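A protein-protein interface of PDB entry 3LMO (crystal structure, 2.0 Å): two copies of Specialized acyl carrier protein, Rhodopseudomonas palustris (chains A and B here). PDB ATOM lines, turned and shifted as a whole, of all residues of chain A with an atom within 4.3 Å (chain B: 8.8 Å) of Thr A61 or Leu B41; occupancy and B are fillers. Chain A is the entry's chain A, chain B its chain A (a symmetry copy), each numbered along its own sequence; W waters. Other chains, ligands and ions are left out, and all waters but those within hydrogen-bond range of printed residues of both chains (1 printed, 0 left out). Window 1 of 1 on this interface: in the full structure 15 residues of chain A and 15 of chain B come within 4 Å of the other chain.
Positions printed for both chains: 57 and 75. Of the 9 pairs that touch across the chains among the printed residues, none has its exchanged pair printed and touching as well.
Water W1 lies within hydrogen-bond range of the backbone carbonyl oxygen (O) of Leu B41 and the side-chain hydroxyl (OG1) of Thr A61.
The side-chain amide oxygen (OD1) of Asn A65 lies close to the side-chain carboxylate (OD1) of Asp B42 (3.4 Å). The side-chain carboxylate (OE2) of Glu A58 lies close to the side-chain carboxylate (OD2) of Asp B48, at 3.4 Å.
O of Leu A57 is in hydrogen-bond range of OG1 of Thr A61. The side-chain amide oxygen (OD1) of Asn A65 sits close to the backbone carbonyl oxygen (O) of Thr A61, 2.8 Å away. N of Leu B38 lies within hydrogen-bond range of OD2 of Asp B36. The side-chain carboxylate (OD1) of Asp B48 is in hydrogen-bond range of the backbone NH (N) of Leu B55 (2.8 Å).
Of the 21 printed residues of chain B, 5 touch a printed residue of chain A. Hydrophobic or aromatic side chains of chain B within 4 Å of the printed part of chain A: Leu B38, Leu B41 and Phe B45. Along chain B the printed residues that touch a printed residue of chain A span positions 38 to 48. Among the printed residues, no Asp or Glu carboxylate lies within 4 Å of a Lys or Arg side-chain nitrogen of the other chain.
Of the printed residues of chain B, Glu A58 touches Phe B45 (3.7 Å) and Asp B48 (3.4 Å). Printed residues of chain B within 4 Å of Phe A75: Leu B38 and Leu B41. Asp B39 touches none of the printed residues of chain A. Of the printed residues of chain A, Phe B45 touches Glu A58, Thr A61 and Gln A62. Ile B47 touches none of the printed residues of chain A. The nearest residue of chain B that does not touch Thr A61 is Leu B38 (6.0 Å). The nearest residue of chain A that does not touch Leu B41 is Leu A57 (4.2 Å). The nearest printed residue of chain B that does not touch Phe A75 is Ser B37 (6.2 Å).
Among the printed residues, pairs that only touch across the chains: Thr A61 with Asp B42 (3.3 Å), Phe A75 with Leu B38 (3.6 Å), Glu A58 with Phe B45 (3.7 Å), Phe A75 with Leu B41 (3.8 Å), Thr A61 with Phe B45 (3.8 Å), Thr A61 with Leu B41 (3.8 Å) and Gln A62 with Phe B45 (3.8 Å).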
ATOM      1  N   LEU A  57      11.104 -23.913 -22.193  1.00  0.00           N
ATOM      2  CA  LEU A  57       9.926 -23.195 -22.656  1.00  0.00           C
ATOM      3  C   LEU A  57      10.116 -22.455 -23.978  1.00  0.00           C
ATOM      4  O   LEU A  57       9.241 -22.490 -24.839  1.00  0.00           O
ATOM      5  CB  LEU A  57       9.461 -22.207 -21.582  1.00  0.00           C
ATOM      6  CG  LEU A  57       9.108 -22.803 -20.208  1.00  0.00           C
ATOM      7  CD1 LEU A  57       8.547 -21.704 -19.301  1.00  0.00           C
ATOM      8  CD2 LEU A  57       8.081 -23.921 -20.376  1.00  0.00           C
ATOM      9  N   GLU A  58      11.249 -21.779 -24.133  1.00  0.00           N
ATOM     10  CA  GLU A  58      11.517 -21.053 -25.368  1.00  0.00           C
ATOM     11  C   GLU A  58      11.558 -22.006 -26.559  1.00  0.00           C
ATOM     12  O   GLU A  58      10.962 -21.739 -27.606  1.00  0.00           O
ATOM     13  CB  GLU A  58      12.844 -20.299 -25.270  1.00  0.00           C
ATOM     14  CG  GLU A  58      13.283 -19.702 -26.593  1.00  0.00           C
ATOM     15  CD  GLU A  58      14.433 -18.732 -26.446  1.00  0.00           C
ATOM     16  OE1 GLU A  58      15.372 -19.035 -25.683  1.00  0.00           O
ATOM     17  OE2 GLU A  58      14.397 -17.672 -27.100  1.00  0.00           O
ATOM     18  N   LYS A  59      12.256 -23.125 -26.390  1.00  0.00           N
ATOM     19  CA  LYS A  59      12.378 -24.116 -27.448  1.00  0.00           C
ATOM     20  C   LYS A  59      11.027 -24.709 -27.838  1.00  0.00           C
ATOM     21  O   LYS A  59      10.752 -24.921 -29.021  1.00  0.00           O
ATOM     22  CB  LYS A  59      13.319 -25.249 -27.018  1.00  0.00           C
ATOM     23  CG  LYS A  59      13.403 -26.391 -28.028  1.00  0.00           C
ATOM     24  CD  LYS A  59      14.163 -27.594 -27.480  1.00  0.00           C
ATOM     25  CE  LYS A  59      14.306 -28.687 -28.545  1.00  0.00           C
ATOM     26  NZ  LYS A  59      14.959 -29.917 -28.016  1.00  0.00           N
ATOM     27  N   TRP A  60      10.193 -24.988 -26.841  1.00  0.00           N
ATOM     28  CA  TRP A  60       8.868 -25.553 -27.085  1.00  0.00           C
ATOM     29  C   TRP A  60       8.013 -24.566 -27.877  1.00  0.00           C
ATOM     30  O   TRP A  60       7.357 -24.937 -28.849  1.00  0.00           O
ATOM     31  CB  TRP A  60       8.183 -25.891 -25.749  1.00  0.00           C
ATOM     32  CG  TRP A  60       8.765 -27.095 -25.029  1.00  0.00           C
ATOM     33  CD1 TRP A  60       9.745 -27.931 -25.484  1.00  0.00           C
ATOM     34  CD2 TRP A  60       8.353 -27.619 -23.756  1.00  0.00           C
ATOM     35  NE1 TRP A  60       9.965 -28.944 -24.579  1.00  0.00           N
ATOM     36  CE2 TRP A  60       9.123 -28.778 -23.511  1.00  0.00           C
ATOM     37  CE3 TRP A  60       7.402 -27.225 -22.806  1.00  0.00           C
ATOM     38  CZ2 TRP A  60       8.976 -29.545 -22.346  1.00  0.00           C
ATOM     39  CZ3 TRP A  60       7.256 -27.988 -21.649  1.00  0.00           C
ATOM     40  CH2 TRP A  60       8.040 -29.136 -21.434  1.00  0.00           C
ATOM     41  N   THR A  61       8.024 -23.305 -27.453  1.00  0.00           N
ATOM     42  CA  THR A  61       7.255 -22.262 -28.133  1.00  0.00           C
ATOM     43  C   THR A  61       7.666 -22.211 -29.607  1.00  0.00           C
ATOM     44  O   THR A  61       6.832 -22.028 -30.491  1.00  0.00           O
ATOM     45  CB  THR A  61       7.508 -20.872 -27.479  1.00  0.00           C
ATOM     46  OG1 THR A  61       7.094 -20.909 -26.105  1.00  0.00           O
ATOM     47  CG2 THR A  61       6.721 -19.771 -28.210  1.00  0.00           C
ATOM     48  N   GLN A  62       8.958 -22.384 -29.869  1.00  0.00           N
ATOM     49  CA  GLN A  62       9.456 -22.348 -31.239  1.00  0.00           C
ATOM     50  C   GLN A  62       8.892 -23.496 -32.085  1.00  0.00           C
ATOM     51  O   GLN A  62       8.555 -23.308 -33.256  1.00  0.00           O
ATOM     52  CB  GLN A  62      10.981 -22.393 -31.238  1.00  0.00           C
ATOM     53  CG  GLN A  62      11.614 -22.266 -32.608  1.00  0.00           C
ATOM     54  CD  GLN A  62      13.106 -22.011 -32.523  1.00  0.00           C
ATOM     55  OE1 GLN A  62      13.854 -22.816 -31.961  1.00  0.00           O
ATOM     56  NE2 GLN A  62      13.547 -20.886 -33.072  1.00  0.00           N
ATOM     57  N   GLU A  63       8.786 -24.680 -31.486  1.00  0.00           N
ATOM     58  CA  GLU A  63       8.261 -25.847 -32.188  1.00  0.00           C
ATOM     59  C   GLU A  63       6.773 -25.705 -32.482  1.00  0.00           C
ATOM     60  O   GLU A  63       6.311 -26.050 -33.570  1.00  0.00           O
ATOM     61  CB  GLU A  63       8.511 -27.118 -31.369  1.00  0.00           C
ATOM     62  CG  GLU A  63       9.986 -27.462 -31.206  1.00  0.00           C
ATOM     63  CD  GLU A  63      10.197 -28.885 -30.724  1.00  0.00           C
ATOM     64  OE1 GLU A  63       9.773 -29.821 -31.437  1.00  0.00           O
ATOM     65  OE2 GLU A  63      10.783 -29.066 -29.636  1.00  0.00           O
ATOM     66  N   VAL A  64       6.021 -25.196 -31.515  1.00  0.00           N
ATOM     67  CA  VAL A  64       4.593 -25.006 -31.708  1.00  0.00           C
ATOM     68  C   VAL A  64       4.342 -23.974 -32.807  1.00  0.00           C
ATOM     69  O   VAL A  64       3.311 -24.018 -33.478  1.00  0.00           O
ATOM     70  CB  VAL A  64       3.902 -24.536 -30.413  1.00  0.00           C
ATOM     71  CG1 VAL A  64       2.437 -24.211 -30.696  1.00  0.00           C
ATOM     72  CG2 VAL A  64       3.991 -25.628 -29.353  1.00  0.00           C
ATOM     73  N   ASN A  65       5.281 -23.047 -32.984  1.00  0.00           N
ATOM     74  CA  ASN A  65       5.152 -22.024 -34.015  1.00  0.00           C
ATOM     75  C   ASN A  65       5.626 -22.527 -35.372  1.00  0.00           C
ATOM     76  O   ASN A  65       5.070 -22.157 -36.403  1.00  0.00           O
ATOM     77  CB  ASN A  65       5.939 -20.762 -33.639  1.00  0.00           C
ATOM     78  CG  ASN A  65       5.172 -19.853 -32.697  1.00  0.00           C
ATOM     79  OD1 ASN A  65       5.176 -20.042 -31.480  1.00  0.00           O
ATOM     80  ND2 ASN A  65       4.490 -18.862 -33.267  1.00  0.00           N
ATOM     81  N   PHE A  75       1.517 -29.321 -22.589  1.00  0.00           N
ATOM     82  CA  PHE A  75       0.648 -28.966 -21.466  1.00  0.00           C
ATOM     83  C   PHE A  75      -0.351 -30.014 -20.938  1.00  0.00           C
ATOM     84  O   PHE A  75      -0.888 -29.849 -19.837  1.00  0.00           O
ATOM     85  CB  PHE A  75      -0.090 -27.671 -21.805  1.00  0.00           C
ATOM     86  CG  PHE A  75       0.828 -26.505 -22.090  1.00  0.00           C
ATOM     87  CD1 PHE A  75       1.341 -25.731 -21.049  1.00  0.00           C
ATOM     88  CD2 PHE A  75       1.189 -26.190 -23.397  1.00  0.00           C
ATOM     89  CE1 PHE A  75       2.200 -24.659 -21.309  1.00  0.00           C
ATOM     90  CE2 PHE A  75       2.046 -25.123 -23.669  1.00  0.00           C
ATOM     91  CZ  PHE A  75       2.554 -24.355 -22.626  1.00  0.00           C
ATOM     92  N   THR B  15       2.542  -9.767 -31.933  1.00  0.00           N
ATOM     93  CA  THR B  15       2.640 -11.167 -31.543  1.00  0.00           C
ATOM     94  C   THR B  15       1.281 -11.747 -31.167  1.00  0.00           C
ATOM     95  O   THR B  15       0.977 -12.893 -31.495  1.00  0.00           O
ATOM     96  CB  THR B  15       3.605 -11.348 -30.348  1.00  0.00           C
ATOM     97  OG1 THR B  15       4.938 -11.011 -30.752  1.00  0.00           O
ATOM     98  CG2 THR B  15       3.583 -12.784 -29.846  1.00  0.00           C
ATOM     99  N   CYS B  16       0.457 -10.951 -30.494  1.00  0.00           N
ATOM    100  CA  CYS B  16      -0.856 -11.418 -30.057  1.00  0.00           C
ATOM    101  C   CYS B  16      -2.013 -10.665 -30.704  1.00  0.00           C
ATOM    102  O   CYS B  16      -3.145 -10.732 -30.225  1.00  0.00           O
ATOM    103  CB  CYS B  16      -0.954 -11.297 -28.537  1.00  0.00           C
ATOM    104  SG  CYS B  16       0.464 -11.978 -27.674  1.00  0.00           S
ATOM    105  N   ALA B  29       2.164  -7.704 -18.860  1.00  0.00           N
ATOM    106  CA  ALA B  29       2.452  -8.708 -19.878  1.00  0.00           C
ATOM    107  C   ALA B  29       1.737 -10.002 -19.513  1.00  0.00           C
ATOM    108  O   ALA B  29       1.761 -10.981 -20.266  1.00  0.00           O
ATOM    109  CB  ALA B  29       3.953  -8.944 -19.962  1.00  0.00           C
ATOM    110  N   ILE B  30       1.095  -9.973 -18.348  1.00  0.00           N
ATOM    111  CA  ILE B  30       0.365 -11.106 -17.807  1.00  0.00           C
ATOM    112  C   ILE B  30      -0.967 -10.646 -17.205  1.00  0.00           C
ATOM    113  O   ILE B  30      -1.063  -9.541 -16.667  1.00  0.00           O
ATOM    114  CB  ILE B  30       1.202 -11.796 -16.705  1.00  0.00           C
ATOM    115  CG1 ILE B  30       1.094 -13.305 -16.850  1.00  0.00           C
ATOM    116  CG2 ILE B  30       0.759 -11.353 -15.318  1.00  0.00           C
ATOM    117  CD1 ILE B  30       1.849 -13.824 -18.030  1.00  0.00           C
ATOM    118  N   ILE B  35      -4.202 -11.279 -22.540  1.00  0.00           N
ATOM    119  CA  ILE B  35      -3.049 -12.161 -22.674  1.00  0.00           C
ATOM    120  C   ILE B  35      -3.154 -13.382 -21.774  1.00  0.00           C
ATOM    121  O   ILE B  35      -3.140 -13.263 -20.549  1.00  0.00           O
ATOM    122  CB  ILE B  35      -1.733 -11.423 -22.325  1.00  0.00           C
ATOM    123  CG1 ILE B  35      -1.550 -10.214 -23.245  1.00  0.00           C
ATOM    124  CG2 ILE B  35      -0.552 -12.371 -22.462  1.00  0.00           C
ATOM    125  CD1 ILE B  35      -0.437  -9.286 -22.816  1.00  0.00           C
ATOM    126  N   ASP B  36      -3.260 -14.556 -22.385  1.00  0.00           N
ATOM    127  CA  ASP B  36      -3.336 -15.791 -21.619  1.00  0.00           C
ATOM    128  C   ASP B  36      -1.935 -16.371 -21.499  1.00  0.00           C
ATOM    129  O   ASP B  36      -0.973 -15.789 -22.006  1.00  0.00           O
ATOM    130  CB  ASP B  36      -4.298 -16.791 -22.285  1.00  0.00           C
ATOM    131  CG  ASP B  36      -3.879 -17.182 -23.693  1.00  0.00           C
ATOM    132  OD1 ASP B  36      -4.758 -17.634 -24.456  1.00  0.00           O
ATOM    133  OD2 ASP B  36      -2.687 -17.058 -24.042  1.00  0.00           O
ATOM    134  N   SER B  37      -1.816 -17.507 -20.825  1.00  0.00           N
ATOM    135  CA  SER B  37      -0.519 -18.136 -20.626  1.00  0.00           C
ATOM    136  C   SER B  37       0.229 -18.432 -21.923  1.00  0.00           C
ATOM    137  O   SER B  37       1.421 -18.145 -22.033  1.00  0.00           O
ATOM    138  CB  SER B  37      -0.683 -19.418 -19.812  1.00  0.00           C
ATOM    139  OG  SER B  37      -1.176 -19.134 -18.516  1.00  0.00           O
ATOM    140  N   LEU B  38      -0.459 -19.009 -22.905  1.00  0.00           N
ATOM    141  CA  LEU B  38       0.193 -19.315 -24.179  1.00  0.00           C
ATOM    142  C   LEU B  38       0.672 -18.023 -24.843  1.00  0.00           C
ATOM    143  O   LEU B  38       1.757 -17.979 -25.419  1.00  0.00           O
ATOM    144  CB  LEU B  38      -0.766 -20.060 -25.113  1.00  0.00           C
ATOM    145  CG  LEU B  38      -1.131 -21.495 -24.727  1.00  0.00           C
ATOM    146  CD1 LEU B  38      -2.265 -21.995 -25.613  1.00  0.00           C
ATOM    147  CD2 LEU B  38       0.096 -22.392 -24.874  1.00  0.00           C
ATOM    148  N   ASP B  39      -0.139 -16.972 -24.752  1.00  0.00           N
ATOM    149  CA  ASP B  39       0.212 -15.683 -25.341  1.00  0.00           C
ATOM    150  C   ASP B  39       1.493 -15.154 -24.713  1.00  0.00           C
ATOM    151  O   ASP B  39       2.396 -14.704 -25.418  1.00  0.00           O
ATOM    152  CB  ASP B  39      -0.907 -14.657 -25.118  1.00  0.00           C
ATOM    153  CG  ASP B  39      -2.167 -14.971 -25.903  1.00  0.00           C
ATOM    154  OD1 ASP B  39      -3.269 -14.720 -25.366  1.00  0.00           O
ATOM    155  OD2 ASP B  39      -2.060 -15.450 -27.056  1.00  0.00           O
ATOM    156  N   PHE B  40       1.571 -15.202 -23.384  1.00  0.00           N
ATOM    157  CA  PHE B  40       2.757 -14.707 -22.688  1.00  0.00           C
ATOM    158  C   PHE B  40       4.030 -15.410 -23.110  1.00  0.00           C
ATOM    159  O   PHE B  40       5.086 -14.774 -23.247  1.00  0.00           O
ATOM    160  CB  PHE B  40       2.619 -14.829 -21.167  1.00  0.00           C
ATOM    161  CG  PHE B  40       3.916 -14.606 -20.429  1.00  0.00           C
ATOM    162  CD1 PHE B  40       4.704 -15.682 -20.031  1.00  0.00           C
ATOM    163  CD2 PHE B  40       4.383 -13.317 -20.189  1.00  0.00           C
ATOM    164  CE1 PHE B  40       5.938 -15.475 -19.409  1.00  0.00           C
ATOM    165  CE2 PHE B  40       5.616 -13.102 -19.569  1.00  0.00           C
ATOM    166  CZ  PHE B  40       6.393 -14.183 -19.179  1.00  0.00           C
ATOM    167  N   LEU B  41       3.950 -16.725 -23.295  1.00  0.00           N
ATOM    168  CA  LEU B  41       5.137 -17.471 -23.708  1.00  0.00           C
ATOM    169  C   LEU B  41       5.558 -17.006 -25.104  1.00  0.00           C
ATOM    170  O   LEU B  41       6.744 -16.970 -25.412  1.00  0.00           O
ATOM    171  CB  LEU B  41       4.862 -18.986 -23.677  1.00  0.00           C
ATOM    172  CG  LEU B  41       4.629 -19.552 -22.265  1.00  0.00           C
ATOM    173  CD1 LEU B  41       4.349 -21.040 -22.334  1.00  0.00           C
ATOM    174  CD2 LEU B  41       5.860 -19.283 -21.403  1.00  0.00           C
ATOM    175  N   ASP B  42       4.588 -16.627 -25.934  1.00  0.00           N
ATOM    176  CA  ASP B  42       4.906 -16.141 -27.273  1.00  0.00           C
ATOM    177  C   ASP B  42       5.587 -14.782 -27.156  1.00  0.00           C
ATOM    178  O   ASP B  42       6.488 -14.457 -27.928  1.00  0.00           O
ATOM    179  CB  ASP B  42       3.645 -16.001 -28.127  1.00  0.00           C
ATOM    180  CG  ASP B  42       3.084 -17.344 -28.569  1.00  0.00           C
ATOM    181  OD1 ASP B  42       3.887 -18.232 -28.924  1.00  0.00           O
ATOM    182  OD2 ASP B  42       1.847 -17.497 -28.579  1.00  0.00           O
ATOM    183  N   ILE B  43       5.150 -13.984 -26.187  1.00  0.00           N
ATOM    184  CA  ILE B  43       5.737 -12.665 -25.979  1.00  0.00           C
ATOM    185  C   ILE B  43       7.180 -12.795 -25.491  1.00  0.00           C
ATOM    186  O   ILE B  43       8.079 -12.118 -25.998  1.00  0.00           O
ATOM    187  CB  ILE B  43       4.908 -11.853 -24.968  1.00  0.00           C
ATOM    188  CG1 ILE B  43       3.531 -11.551 -25.578  1.00  0.00           C
ATOM    189  CG2 ILE B  43       5.637 -10.551 -24.607  1.00  0.00           C
ATOM    190  CD1 ILE B  43       2.518 -11.002 -24.593  1.00  0.00           C
ATOM    191  N   ALA B  44       7.407 -13.670 -24.516  1.00  0.00           N
ATOM    192  CA  ALA B  44       8.750 -13.877 -23.985  1.00  0.00           C
ATOM    193  C   ALA B  44       9.666 -14.356 -25.112  1.00  0.00           C
ATOM    194  O   ALA B  44      10.821 -13.948 -25.197  1.00  0.00           O
ATOM    195  CB  ALA B  44       8.717 -14.915 -22.857  1.00  0.00           C
ATOM    196  N   PHE B  45       9.140 -15.226 -25.972  1.00  0.00           N
ATOM    197  CA  PHE B  45       9.907 -15.753 -27.102  1.00  0.00           C
ATOM    198  C   PHE B  45      10.278 -14.599 -28.037  1.00  0.00           C
ATOM    199  O   PHE B  45      11.446 -14.405 -28.365  1.00  0.00           O
ATOM    200  CB  PHE B  45       9.084 -16.804 -27.864  1.00  0.00           C
ATOM    201  CG  PHE B  45       9.802 -17.402 -29.058  1.00  0.00           C
ATOM    202  CD1 PHE B  45       9.166 -17.496 -30.291  1.00  0.00           C
ATOM    203  CD2 PHE B  45      11.109 -17.871 -28.946  1.00  0.00           C
ATOM    204  CE1 PHE B  45       9.822 -18.048 -31.401  1.00  0.00           C
ATOM    205  CE2 PHE B  45      11.775 -18.426 -30.048  1.00  0.00           C
ATOM    206  CZ  PHE B  45      11.130 -18.513 -31.275  1.00  0.00           C
ATOM    207  N   ALA B  46       9.278 -13.830 -28.450  1.00  0.00           N
ATOM    208  CA  ALA B  46       9.511 -12.704 -29.350  1.00  0.00           C
ATOM    209  C   ALA B  46      10.508 -11.689 -28.779  1.00  0.00           C
ATOM    210  O   ALA B  46      11.369 -11.184 -29.498  1.00  0.00           O
ATOM    211  CB  ALA B  46       8.192 -12.017 -29.676  1.00  0.00           C
ATOM    212  N   ILE B  47      10.395 -11.392 -27.488  1.00  0.00           N
ATOM    213  CA  ILE B  47      11.304 -10.439 -26.852  1.00  0.00           C
ATOM    214  C   ILE B  47      12.752 -10.942 -26.883  1.00  0.00           C
ATOM    215  O   ILE B  47      13.679 -10.188 -27.195  1.00  0.00           O
ATOM    216  CB  ILE B  47      10.872 -10.162 -25.393  1.00  0.00           C
ATOM    217  CG1 ILE B  47       9.589  -9.319 -25.401  1.00  0.00           C
ATOM    218  CG2 ILE B  47      11.998  -9.484 -24.618  1.00  0.00           C
ATOM    219  CD1 ILE B  47       8.995  -9.069 -24.025  1.00  0.00           C
ATOM    220  N   ASP B  48      12.937 -12.217 -26.559  1.00  0.00           N
ATOM    221  CA  ASP B  48      14.263 -12.830 -26.562  1.00  0.00           C
ATOM    222  C   ASP B  48      14.954 -12.629 -27.904  1.00  0.00           C
ATOM    223  O   ASP B  48      16.069 -12.140 -27.953  1.00  0.00           O
ATOM    224  CB  ASP B  48      14.161 -14.334 -26.292  1.00  0.00           C
ATOM    225  CG  ASP B  48      13.587 -14.644 -24.930  1.00  0.00           C
ATOM    226  OD1 ASP B  48      13.829 -13.847 -23.991  1.00  0.00           O
ATOM    227  OD2 ASP B  48      12.917 -15.691 -24.797  1.00  0.00           O
ATOM    228  N   LEU B  55      14.881 -13.997 -21.407  1.00  0.00           N
ATOM    229  CA  LEU B  55      14.214 -13.627 -20.164  1.00  0.00           C
ATOM    230  C   LEU B  55      14.336 -14.853 -19.270  1.00  0.00           C
ATOM    231  O   LEU B  55      13.725 -15.885 -19.527  1.00  0.00           O
ATOM    232  CB  LEU B  55      12.743 -13.297 -20.405  1.00  0.00           C
ATOM    233  CG  LEU B  55      12.458 -12.135 -21.358  1.00  0.00           C
ATOM    234  CD1 LEU B  55      10.957 -11.983 -21.513  1.00  0.00           C
ATOM    235  CD2 LEU B  55      13.090 -10.854 -20.829  1.00  0.00           C
ATOM    236  N   LEU B  57      13.081 -16.662 -16.916  1.00  0.00           N
ATOM    237  CA  LEU B  57      11.847 -16.915 -16.188  1.00  0.00           C
ATOM    238  C   LEU B  57      12.024 -17.725 -14.907  1.00  0.00           C
ATOM    239  O   LEU B  57      11.424 -17.407 -13.883  1.00  0.00           O
ATOM    240  CB  LEU B  57      10.838 -17.618 -17.100  1.00  0.00           C
ATOM    241  CG  LEU B  57      10.450 -16.880 -18.393  1.00  0.00           C
ATOM    242  CD1 LEU B  57       9.347 -17.658 -19.117  1.00  0.00           C
ATOM    243  CD2 LEU B  57       9.964 -15.470 -18.059  1.00  0.00           C
ATOM    244  N   PHE B  75       6.466  -8.130 -14.741  1.00  0.00           N
ATOM    245  CA  PHE B  75       5.311  -8.095 -15.641  1.00  0.00           C
ATOM    246  C   PHE B  75       4.681  -6.733 -15.990  1.00  0.00           C
ATOM    247  O   PHE B  75       3.904  -6.645 -16.946  1.00  0.00           O
ATOM    248  CB  PHE B  75       4.238  -9.041 -15.103  1.00  0.00           C
ATOM    249  CG  PHE B  75       4.701 -10.472 -14.970  1.00  0.00           C
ATOM    250  CD1 PHE B  75       4.663 -11.340 -16.063  1.00  0.00           C
ATOM    251  CD2 PHE B  75       5.186 -10.952 -13.755  1.00  0.00           C
ATOM    252  CE1 PHE B  75       5.102 -12.661 -15.945  1.00  0.00           C
ATOM    253  CE2 PHE B  75       5.627 -12.269 -13.626  1.00  0.00           C
ATOM    254  CZ  PHE B  75       5.587 -13.126 -14.721  1.00  0.00           C
HETATM  255  O   HOH W   1       8.461 -18.876 -24.553  1.00  0.00           O
